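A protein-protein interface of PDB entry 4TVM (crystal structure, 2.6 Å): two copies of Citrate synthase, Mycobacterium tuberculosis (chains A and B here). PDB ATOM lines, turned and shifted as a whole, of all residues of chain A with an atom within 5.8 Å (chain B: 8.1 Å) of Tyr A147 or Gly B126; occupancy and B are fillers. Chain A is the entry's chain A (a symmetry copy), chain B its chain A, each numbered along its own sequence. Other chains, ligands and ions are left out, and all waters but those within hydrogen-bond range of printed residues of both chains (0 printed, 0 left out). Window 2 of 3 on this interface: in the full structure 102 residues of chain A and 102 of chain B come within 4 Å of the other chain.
Phe A123 touches its own counterpart, Phe B123.
Of the 9 pairs that touch across the chains among the printed residues, 1 has its exchanged pair printed and touching as well.
Among the printed residues, pairs that only touch across the chains: Phe A123 with Phe B123, Phe A123 with Phe B127, Phe A123 with Ser B139, Ala A143 with Ser B139, Tyr A147 with Pro B128, Phe A123 with Gly B126, Ala A146 with Pro B128 and Ala A143 with Phe B127.
Of the 13 printed residues of chain B, 5 touch a printed residue of chain A.
Printed residues of chain B that touch a printed residue of chain A: Phe B123, Gly B126, Phe B127, Pro B128 and Ser B139.
Hydrophobic or aromatic side chains of chain B within 4 Å of the printed part of chain A: Phe B123, Phe B127 and Pro B128.
Tyr A147 touches two residues of chain B.
Gly B126 touches just these residues of chain A: Phe A123 and Tyr A147.
Of the printed residues of chain B, Ala A143 touches Phe B127 (3.98 Å) and Ser B139 (3.6 Å).
Of the printed residues of chain B, Phe A123 touches Phe B123 (3.0 Å), Gly B126 (3.8 Å), Phe B127 (3.3 Å) and Ser B139 (3.6 Å).
Of the printed residues of chain A, Phe B123 touches Phe A123 (3.0 Å).
The nearest residue of chain A that does not touch Gly B126 is Asp A119 (4.5 Å).
O of Gly B126 is in hydrogen-bond range of OH of Tyr A147 (3.0 Å).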
ATOM      1  N   HIS A 117      -6.338  24.822  26.951  1.00  0.00           N
ATOM      2  CA  HIS A 117      -5.049  25.506  26.738  1.00  0.00           C
ATOM      3  C   HIS A 117      -4.972  26.024  25.317  1.00  0.00           C
ATOM      4  O   HIS A 117      -5.152  25.244  24.370  1.00  0.00           O
ATOM      5  CB  HIS A 117      -3.872  24.524  26.957  1.00  0.00           C
ATOM      6  CG  HIS A 117      -2.593  25.204  27.325  1.00  0.00           C
ATOM      7  ND1 HIS A 117      -1.787  25.827  26.394  1.00  0.00           N
ATOM      8  CD2 HIS A 117      -1.981  25.368  28.520  1.00  0.00           C
ATOM      9  CE1 HIS A 117      -0.736  26.344  26.997  1.00  0.00           C
ATOM     10  NE2 HIS A 117      -0.838  26.084  28.290  1.00  0.00           N
ATOM     11  N   ASP A 119      -2.546  26.547  23.366  1.00  0.00           N
ATOM     12  CA  ASP A 119      -1.707  25.688  22.525  1.00  0.00           C
ATOM     13  C   ASP A 119      -2.435  24.442  22.033  1.00  0.00           C
ATOM     14  O   ASP A 119      -2.247  24.003  20.892  1.00  0.00           O
ATOM     15  CB  ASP A 119      -0.450  25.269  23.250  1.00  0.00           C
ATOM     16  CG  ASP A 119       0.550  26.380  23.397  1.00  0.00           C
ATOM     17  OD1 ASP A 119       0.289  27.530  22.990  1.00  0.00           O
ATOM     18  OD2 ASP A 119       1.622  26.086  23.953  1.00  0.00           O
ATOM     19  N   LEU A 120      -3.269  23.872  22.893  1.00  0.00           N
ATOM     20  CA  LEU A 120      -4.092  22.725  22.509  1.00  0.00           C
ATOM     21  C   LEU A 120      -5.152  23.141  21.549  1.00  0.00           C
ATOM     22  O   LEU A 120      -5.506  22.396  20.647  1.00  0.00           O
ATOM     23  CB  LEU A 120      -4.729  22.031  23.702  1.00  0.00           C
ATOM     24  CG  LEU A 120      -5.484  20.772  23.267  1.00  0.00           C
ATOM     25  CD1 LEU A 120      -4.520  19.744  22.721  1.00  0.00           C
ATOM     26  CD2 LEU A 120      -6.324  20.176  24.387  1.00  0.00           C
ATOM     27  N   PHE A 123      -3.075  23.535  18.219  1.00  0.00           N
ATOM     28  CA  PHE A 123      -2.785  22.195  17.713  1.00  0.00           C
ATOM     29  C   PHE A 123      -3.789  21.657  16.697  1.00  0.00           C
ATOM     30  O   PHE A 123      -3.440  20.832  15.877  1.00  0.00           O
ATOM     31  CB  PHE A 123      -2.755  21.278  18.918  1.00  0.00           C
ATOM     32  CG  PHE A 123      -2.427  19.847  18.624  1.00  0.00           C
ATOM     33  CD1 PHE A 123      -3.435  18.938  18.367  1.00  0.00           C
ATOM     34  CD2 PHE A 123      -1.129  19.393  18.735  1.00  0.00           C
ATOM     35  CE1 PHE A 123      -3.154  17.597  18.162  1.00  0.00           C
ATOM     36  CE2 PHE A 123      -0.830  18.054  18.521  1.00  0.00           C
ATOM     37  CZ  PHE A 123      -1.850  17.149  18.243  1.00  0.00           C
ATOM     38  N   ALA A 143      -3.388  13.677  23.053  1.00  0.00           N
ATOM     39  CA  ALA A 143      -2.563  14.854  23.316  1.00  0.00           C
ATOM     40  C   ALA A 143      -2.862  15.548  24.666  1.00  0.00           C
ATOM     41  O   ALA A 143      -2.070  16.383  25.152  1.00  0.00           O
ATOM     42  CB  ALA A 143      -2.710  15.840  22.173  1.00  0.00           C
ATOM     43  N   LEU A 144      -3.992  15.237  25.277  1.00  0.00           N
ATOM     44  CA  LEU A 144      -4.339  15.832  26.581  1.00  0.00           C
ATOM     45  C   LEU A 144      -3.297  15.579  27.641  1.00  0.00           C
ATOM     46  O   LEU A 144      -3.109  16.404  28.529  1.00  0.00           O
ATOM     47  CB  LEU A 144      -5.631  15.219  27.117  1.00  0.00           C
ATOM     48  CG  LEU A 144      -6.883  15.711  26.443  1.00  0.00           C
ATOM     49  CD1 LEU A 144      -8.032  14.788  26.798  1.00  0.00           C
ATOM     50  CD2 LEU A 144      -7.175  17.144  26.893  1.00  0.00           C
ATOM     51  N   SER A 145      -2.685  14.400  27.594  1.00  0.00           N
ATOM     52  CA  SER A 145      -1.679  14.043  28.554  1.00  0.00           C
ATOM     53  C   SER A 145      -0.457  14.937  28.367  1.00  0.00           C
ATOM     54  O   SER A 145       0.316  15.140  29.292  1.00  0.00           O
ATOM     55  CB  SER A 145      -1.299  12.580  28.403  1.00  0.00           C
ATOM     56  OG  SER A 145      -2.396  11.741  28.726  1.00  0.00           O
ATOM     57  N   ALA A 146      -0.297  15.494  27.174  1.00  0.00           N
ATOM     58  CA  ALA A 146       0.739  16.484  26.936  1.00  0.00           C
ATOM     59  C   ALA A 146       0.461  17.835  27.615  1.00  0.00           C
ATOM     60  O   ALA A 146       1.393  18.591  27.859  1.00  0.00           O
ATOM     61  CB  ALA A 146       0.945  16.689  25.427  1.00  0.00           C
ATOM     62  N   TYR A 147      -0.799  18.178  27.870  1.00  0.00           N
ATOM     63  CA  TYR A 147      -1.113  19.519  28.406  1.00  0.00           C
ATOM     64  C   TYR A 147      -1.607  19.510  29.839  1.00  0.00           C
ATOM     65  O   TYR A 147      -1.643  20.540  30.503  1.00  0.00           O
ATOM     66  CB  TYR A 147      -2.158  20.199  27.541  1.00  0.00           C
ATOM     67  CG  TYR A 147      -1.669  20.509  26.186  1.00  0.00           C
ATOM     68  CD1 TYR A 147      -1.793  19.575  25.156  1.00  0.00           C
ATOM     69  CD2 TYR A 147      -1.041  21.718  25.917  1.00  0.00           C
ATOM     70  CE1 TYR A 147      -1.310  19.845  23.875  1.00  0.00           C
ATOM     71  CE2 TYR A 147      -0.551  21.996  24.636  1.00  0.00           C
ATOM     72  CZ  TYR A 147      -0.700  21.066  23.628  1.00  0.00           C
ATOM     73  OH  TYR A 147      -0.245  21.343  22.377  1.00  0.00           O
ATOM     74  N   TYR A 148      -2.046  18.353  30.296  1.00  0.00           N
ATOM     75  CA  TYR A 148      -2.603  18.222  31.616  1.00  0.00           C
ATOM     76  C   TYR A 148      -1.849  17.065  32.264  1.00  0.00           C
ATOM     77  O   TYR A 148      -2.441  16.108  32.741  1.00  0.00           O
ATOM     78  CB  TYR A 148      -4.139  18.036  31.513  1.00  0.00           C
ATOM     79  CG  TYR A 148      -4.786  19.214  30.772  1.00  0.00           C
ATOM     80  CD1 TYR A 148      -5.118  20.386  31.435  1.00  0.00           C
ATOM     81  CD2 TYR A 148      -5.023  19.171  29.400  1.00  0.00           C
ATOM     82  CE1 TYR A 148      -5.692  21.479  30.771  1.00  0.00           C
ATOM     83  CE2 TYR A 148      -5.591  20.249  28.730  1.00  0.00           C
ATOM     84  CZ  TYR A 148      -5.912  21.417  29.418  1.00  0.00           C
ATOM     85  OH  TYR A 148      -6.448  22.530  28.734  1.00  0.00           O
ATOM     86  N   GLN A 149      -0.513  17.189  32.227  1.00  0.00           N
ATOM     87  CA  GLN A 149       0.450  16.353  32.970  1.00  0.00           C
ATOM     88  C   GLN A 149       0.183  16.511  34.459  1.00  0.00           C
ATOM     89  O   GLN A 149       0.512  15.673  35.284  1.00  0.00           O
ATOM     90  CB  GLN A 149       1.882  16.856  32.722  1.00  0.00           C
ATOM     91  CG  GLN A 149       2.363  16.831  31.291  1.00  0.00           C
ATOM     92  CD  GLN A 149       3.820  17.233  31.159  1.00  0.00           C
ATOM     93  OE1 GLN A 149       4.239  18.276  31.662  1.00  0.00           O
ATOM     94  NE2 GLN A 149       4.604  16.408  30.467  1.00  0.00           N
ATOM     95  N   ASP A 150      -0.351  17.671  34.768  1.00  0.00           N
ATOM     96  CA  ASP A 150      -0.807  18.065  36.076  1.00  0.00           C
ATOM     97  C   ASP A 150      -1.380  16.956  37.002  1.00  0.00           C
ATOM     98  O   ASP A 150      -0.966  16.848  38.146  1.00  0.00           O
ATOM     99  CB  ASP A 150      -1.888  19.139  35.832  1.00  0.00           C
ATOM    100  CG  ASP A 150      -2.050  20.063  36.976  1.00  0.00           C
ATOM    101  OD1 ASP A 150      -1.534  19.763  38.065  1.00  0.00           O
ATOM    102  OD2 ASP A 150      -2.697  21.106  36.788  1.00  0.00           O
ATOM    103  N   LYS B 121       4.711  15.488   9.351  1.00  0.00           N
ATOM    104  CA  LYS B 121       5.968  15.926   9.985  1.00  0.00           C
ATOM    105  C   LYS B 121       5.794  17.216  10.743  1.00  0.00           C
ATOM    106  O   LYS B 121       6.146  17.288  11.904  1.00  0.00           O
ATOM    107  CB  LYS B 121       7.034  16.127   8.930  1.00  0.00           C
ATOM    108  CG  LYS B 121       8.442  16.166   9.467  1.00  0.00           C
ATOM    109  CD  LYS B 121       9.368  16.843   8.480  1.00  0.00           C
ATOM    110  CE  LYS B 121      10.812  16.802   8.944  1.00  0.00           C
ATOM    111  NZ  LYS B 121      11.451  18.125   8.800  1.00  0.00           N
ATOM    112  N   ARG B 122       5.228  18.232  10.077  1.00  0.00           N
ATOM    113  CA  ARG B 122       4.992  19.547  10.677  1.00  0.00           C
ATOM    114  C   ARG B 122       4.103  19.506  11.925  1.00  0.00           C
ATOM    115  O   ARG B 122       4.334  20.233  12.869  1.00  0.00           O
ATOM    116  CB  ARG B 122       4.355  20.472   9.648  1.00  0.00           C
ATOM    117  CG  ARG B 122       5.322  21.144   8.682  1.00  0.00           C
ATOM    118  CD  ARG B 122       4.573  21.694   7.469  1.00  0.00           C
ATOM    119  NE  ARG B 122       3.408  22.490   7.859  1.00  0.00           N
ATOM    120  CZ  ARG B 122       2.563  23.071   7.003  1.00  0.00           C
ATOM    121  NH1 ARG B 122       2.736  22.959   5.685  1.00  0.00           N
ATOM    122  NH2 ARG B 122       1.539  23.781   7.471  1.00  0.00           N
ATOM    123  N   PHE B 123       3.069  18.670  11.899  1.00  0.00           N
ATOM    124  CA  PHE B 123       2.167  18.433  13.025  1.00  0.00           C
ATOM    125  C   PHE B 123       2.858  18.161  14.359  1.00  0.00           C
ATOM    126  O   PHE B 123       2.290  18.422  15.400  1.00  0.00           O
ATOM    127  CB  PHE B 123       1.318  17.236  12.650  1.00  0.00           C
ATOM    128  CG  PHE B 123       0.283  16.846  13.660  1.00  0.00           C
ATOM    129  CD1 PHE B 123       0.579  15.917  14.639  1.00  0.00           C
ATOM    130  CD2 PHE B 123      -1.011  17.309  13.545  1.00  0.00           C
ATOM    131  CE1 PHE B 123      -0.387  15.493  15.537  1.00  0.00           C
ATOM    132  CE2 PHE B 123      -1.987  16.902  14.445  1.00  0.00           C
ATOM    133  CZ  PHE B 123      -1.676  15.980  15.440  1.00  0.00           C
ATOM    134  N   PHE B 124       4.097  17.663  14.331  1.00  0.00           N
ATOM    135  CA  PHE B 124       4.913  17.610  15.548  1.00  0.00           C
ATOM    136  C   PHE B 124       5.170  18.986  16.151  1.00  0.00           C
ATOM    137  O   PHE B 124       5.482  19.108  17.347  1.00  0.00           O
ATOM    138  CB  PHE B 124       6.244  16.889  15.292  1.00  0.00           C
ATOM    139  CG  PHE B 124       6.123  15.361  15.239  1.00  0.00           C
ATOM    140  CD1 PHE B 124       5.795  14.706  14.052  1.00  0.00           C
ATOM    141  CD2 PHE B 124       6.351  14.600  16.368  1.00  0.00           C
ATOM    142  CE1 PHE B 124       5.699  13.329  13.991  1.00  0.00           C
ATOM    143  CE2 PHE B 124       6.276  13.225  16.322  1.00  0.00           C
ATOM    144  CZ  PHE B 124       5.948  12.583  15.129  1.00  0.00           C
ATOM    145  N   ASP B 125       5.010  20.021  15.334  1.00  0.00           N
ATOM    146  CA  ASP B 125       5.272  21.380  15.773  1.00  0.00           C
ATOM    147  C   ASP B 125       4.311  21.881  16.839  1.00  0.00           C
ATOM    148  O   ASP B 125       4.670  22.747  17.639  1.00  0.00           O
ATOM    149  CB  ASP B 125       5.292  22.335  14.568  1.00  0.00           C
ATOM    150  CG  ASP B 125       6.515  22.124  13.689  1.00  0.00           C
ATOM    151  OD1 ASP B 125       7.385  21.319  14.081  1.00  0.00           O
ATOM    152  OD2 ASP B 125       6.617  22.753  12.611  1.00  0.00           O
ATOM    153  N   GLY B 126       3.106  21.318  16.858  1.00  0.00           N
ATOM    154  CA  GLY B 126       2.055  21.743  17.772  1.00  0.00           C
ATOM    155  C   GLY B 126       2.195  21.240  19.187  1.00  0.00           C
ATOM    156  O   GLY B 126       1.618  21.807  20.135  1.00  0.00           O
ATOM    157  N   PHE B 127       2.939  20.163  19.370  1.00  0.00           N
ATOM    158  CA  PHE B 127       3.173  19.680  20.726  1.00  0.00           C
ATOM    159  C   PHE B 127       4.052  20.665  21.521  1.00  0.00           C
ATOM    160  O   PHE B 127       4.782  21.481  20.942  1.00  0.00           O
ATOM    161  CB  PHE B 127       3.789  18.279  20.683  1.00  0.00           C
ATOM    162  CG  PHE B 127       2.843  17.239  20.159  1.00  0.00           C
ATOM    163  CD1 PHE B 127       1.731  16.852  20.903  1.00  0.00           C
ATOM    164  CD2 PHE B 127       3.049  16.642  18.927  1.00  0.00           C
ATOM    165  CE1 PHE B 127       0.867  15.881  20.420  1.00  0.00           C
ATOM    166  CE2 PHE B 127       2.167  15.680  18.434  1.00  0.00           C
ATOM    167  CZ  PHE B 127       1.075  15.309  19.174  1.00  0.00           C
ATOM    168  N   PRO B 128       3.971  20.599  22.853  1.00  0.00           N
ATOM    169  CA  PRO B 128       4.673  21.510  23.755  1.00  0.00           C
ATOM    170  C   PRO B 128       6.159  21.268  23.734  1.00  0.00           C
ATOM    171  O   PRO B 128       6.583  20.260  23.170  1.00  0.00           O
ATOM    172  CB  PRO B 128       4.105  21.176  25.119  1.00  0.00           C
ATOM    173  CG  PRO B 128       2.846  20.485  24.856  1.00  0.00           C
ATOM    174  CD  PRO B 128       2.932  19.819  23.531  1.00  0.00           C
ATOM    175  N   ARG B 129       6.921  22.137  24.406  1.00  0.00           N
ATOM    176  CA  ARG B 129       8.334  22.350  24.085  1.00  0.00           C
ATOM    177  C   ARG B 129       9.239  21.122  24.169  1.00  0.00           C
ATOM    178  O   ARG B 129      10.071  20.918  23.271  1.00  0.00           O
ATOM    179  CB  ARG B 129       8.945  23.516  24.890  1.00  0.00           C
ATOM    180  CG  ARG B 129      10.407  23.788  24.552  1.00  0.00           C
ATOM    181  CD  ARG B 129      10.897  25.105  25.093  1.00  0.00           C
ATOM    182  NE  ARG B 129      10.851  25.142  26.556  1.00  0.00           N
ATOM    183  CZ  ARG B 129      11.829  24.714  27.352  1.00  0.00           C
ATOM    184  NH1 ARG B 129      12.954  24.195  26.854  1.00  0.00           N
ATOM    185  NH2 ARG B 129      11.684  24.812  28.670  1.00  0.00           N
ATOM    186  N   ALA B 131       7.945  17.583  25.057  1.00  0.00           N
ATOM    187  CA  ALA B 131       6.888  16.712  25.533  1.00  0.00           C
ATOM    188  C   ALA B 131       7.299  15.249  25.506  1.00  0.00           C
ATOM    189  O   ALA B 131       8.117  14.829  24.683  1.00  0.00           O
ATOM    190  CB  ALA B 131       5.637  16.918  24.693  1.00  0.00           C
ATOM    191  N   PRO B 135       3.074  10.255  24.771  1.00  0.00           N
ATOM    192  CA  PRO B 135       1.886  11.003  24.366  1.00  0.00           C
ATOM    193  C   PRO B 135       1.858  11.406  22.902  1.00  0.00           C
ATOM    194  O   PRO B 135       0.828  11.311  22.235  1.00  0.00           O
ATOM    195  CB  PRO B 135       1.957  12.265  25.233  1.00  0.00           C
ATOM    196  CG  PRO B 135       2.704  11.859  26.447  1.00  0.00           C
ATOM    197  CD  PRO B 135       3.543  10.658  26.106  1.00  0.00           C
ATOM    198  N   SER B 139      -0.747  10.283  19.819  1.00  0.00           N
ATOM    199  CA  SER B 139      -1.459  11.353  19.182  1.00  0.00           C
ATOM    200  C   SER B 139      -1.283  11.243  17.684  1.00  0.00           C
ATOM    201  O   SER B 139      -2.249  11.374  16.928  1.00  0.00           O
ATOM    202  CB  SER B 139      -0.958  12.688  19.705  1.00  0.00           C
ATOM    203  OG  SER B 139      -1.846  13.729  19.373  1.00  0.00           O
ATOM    204  N   LYS B 181      11.616  15.610  19.428  1.00  0.00           N
ATOM    205  CA  LYS B 181      10.750  16.597  20.022  1.00  0.00           C
ATOM    206  C   LYS B 181      10.946  16.691  21.527  1.00  0.00           C
ATOM    207  O   LYS B 181      10.889  17.768  22.088  1.00  0.00           O
ATOM    208  CB  LYS B 181       9.300  16.262  19.713  1.00  0.00           C
ATOM    209  CG  LYS B 181       8.309  17.366  20.105  1.00  0.00           C
ATOM    210  CD  LYS B 181       8.552  18.632  19.302  1.00  0.00           C
ATOM    211  CE  LYS B 181       7.874  19.828  19.937  1.00  0.00           C
ATOM    212  NZ  LYS B 181       8.034  21.006  19.029  1.00  0.00           N
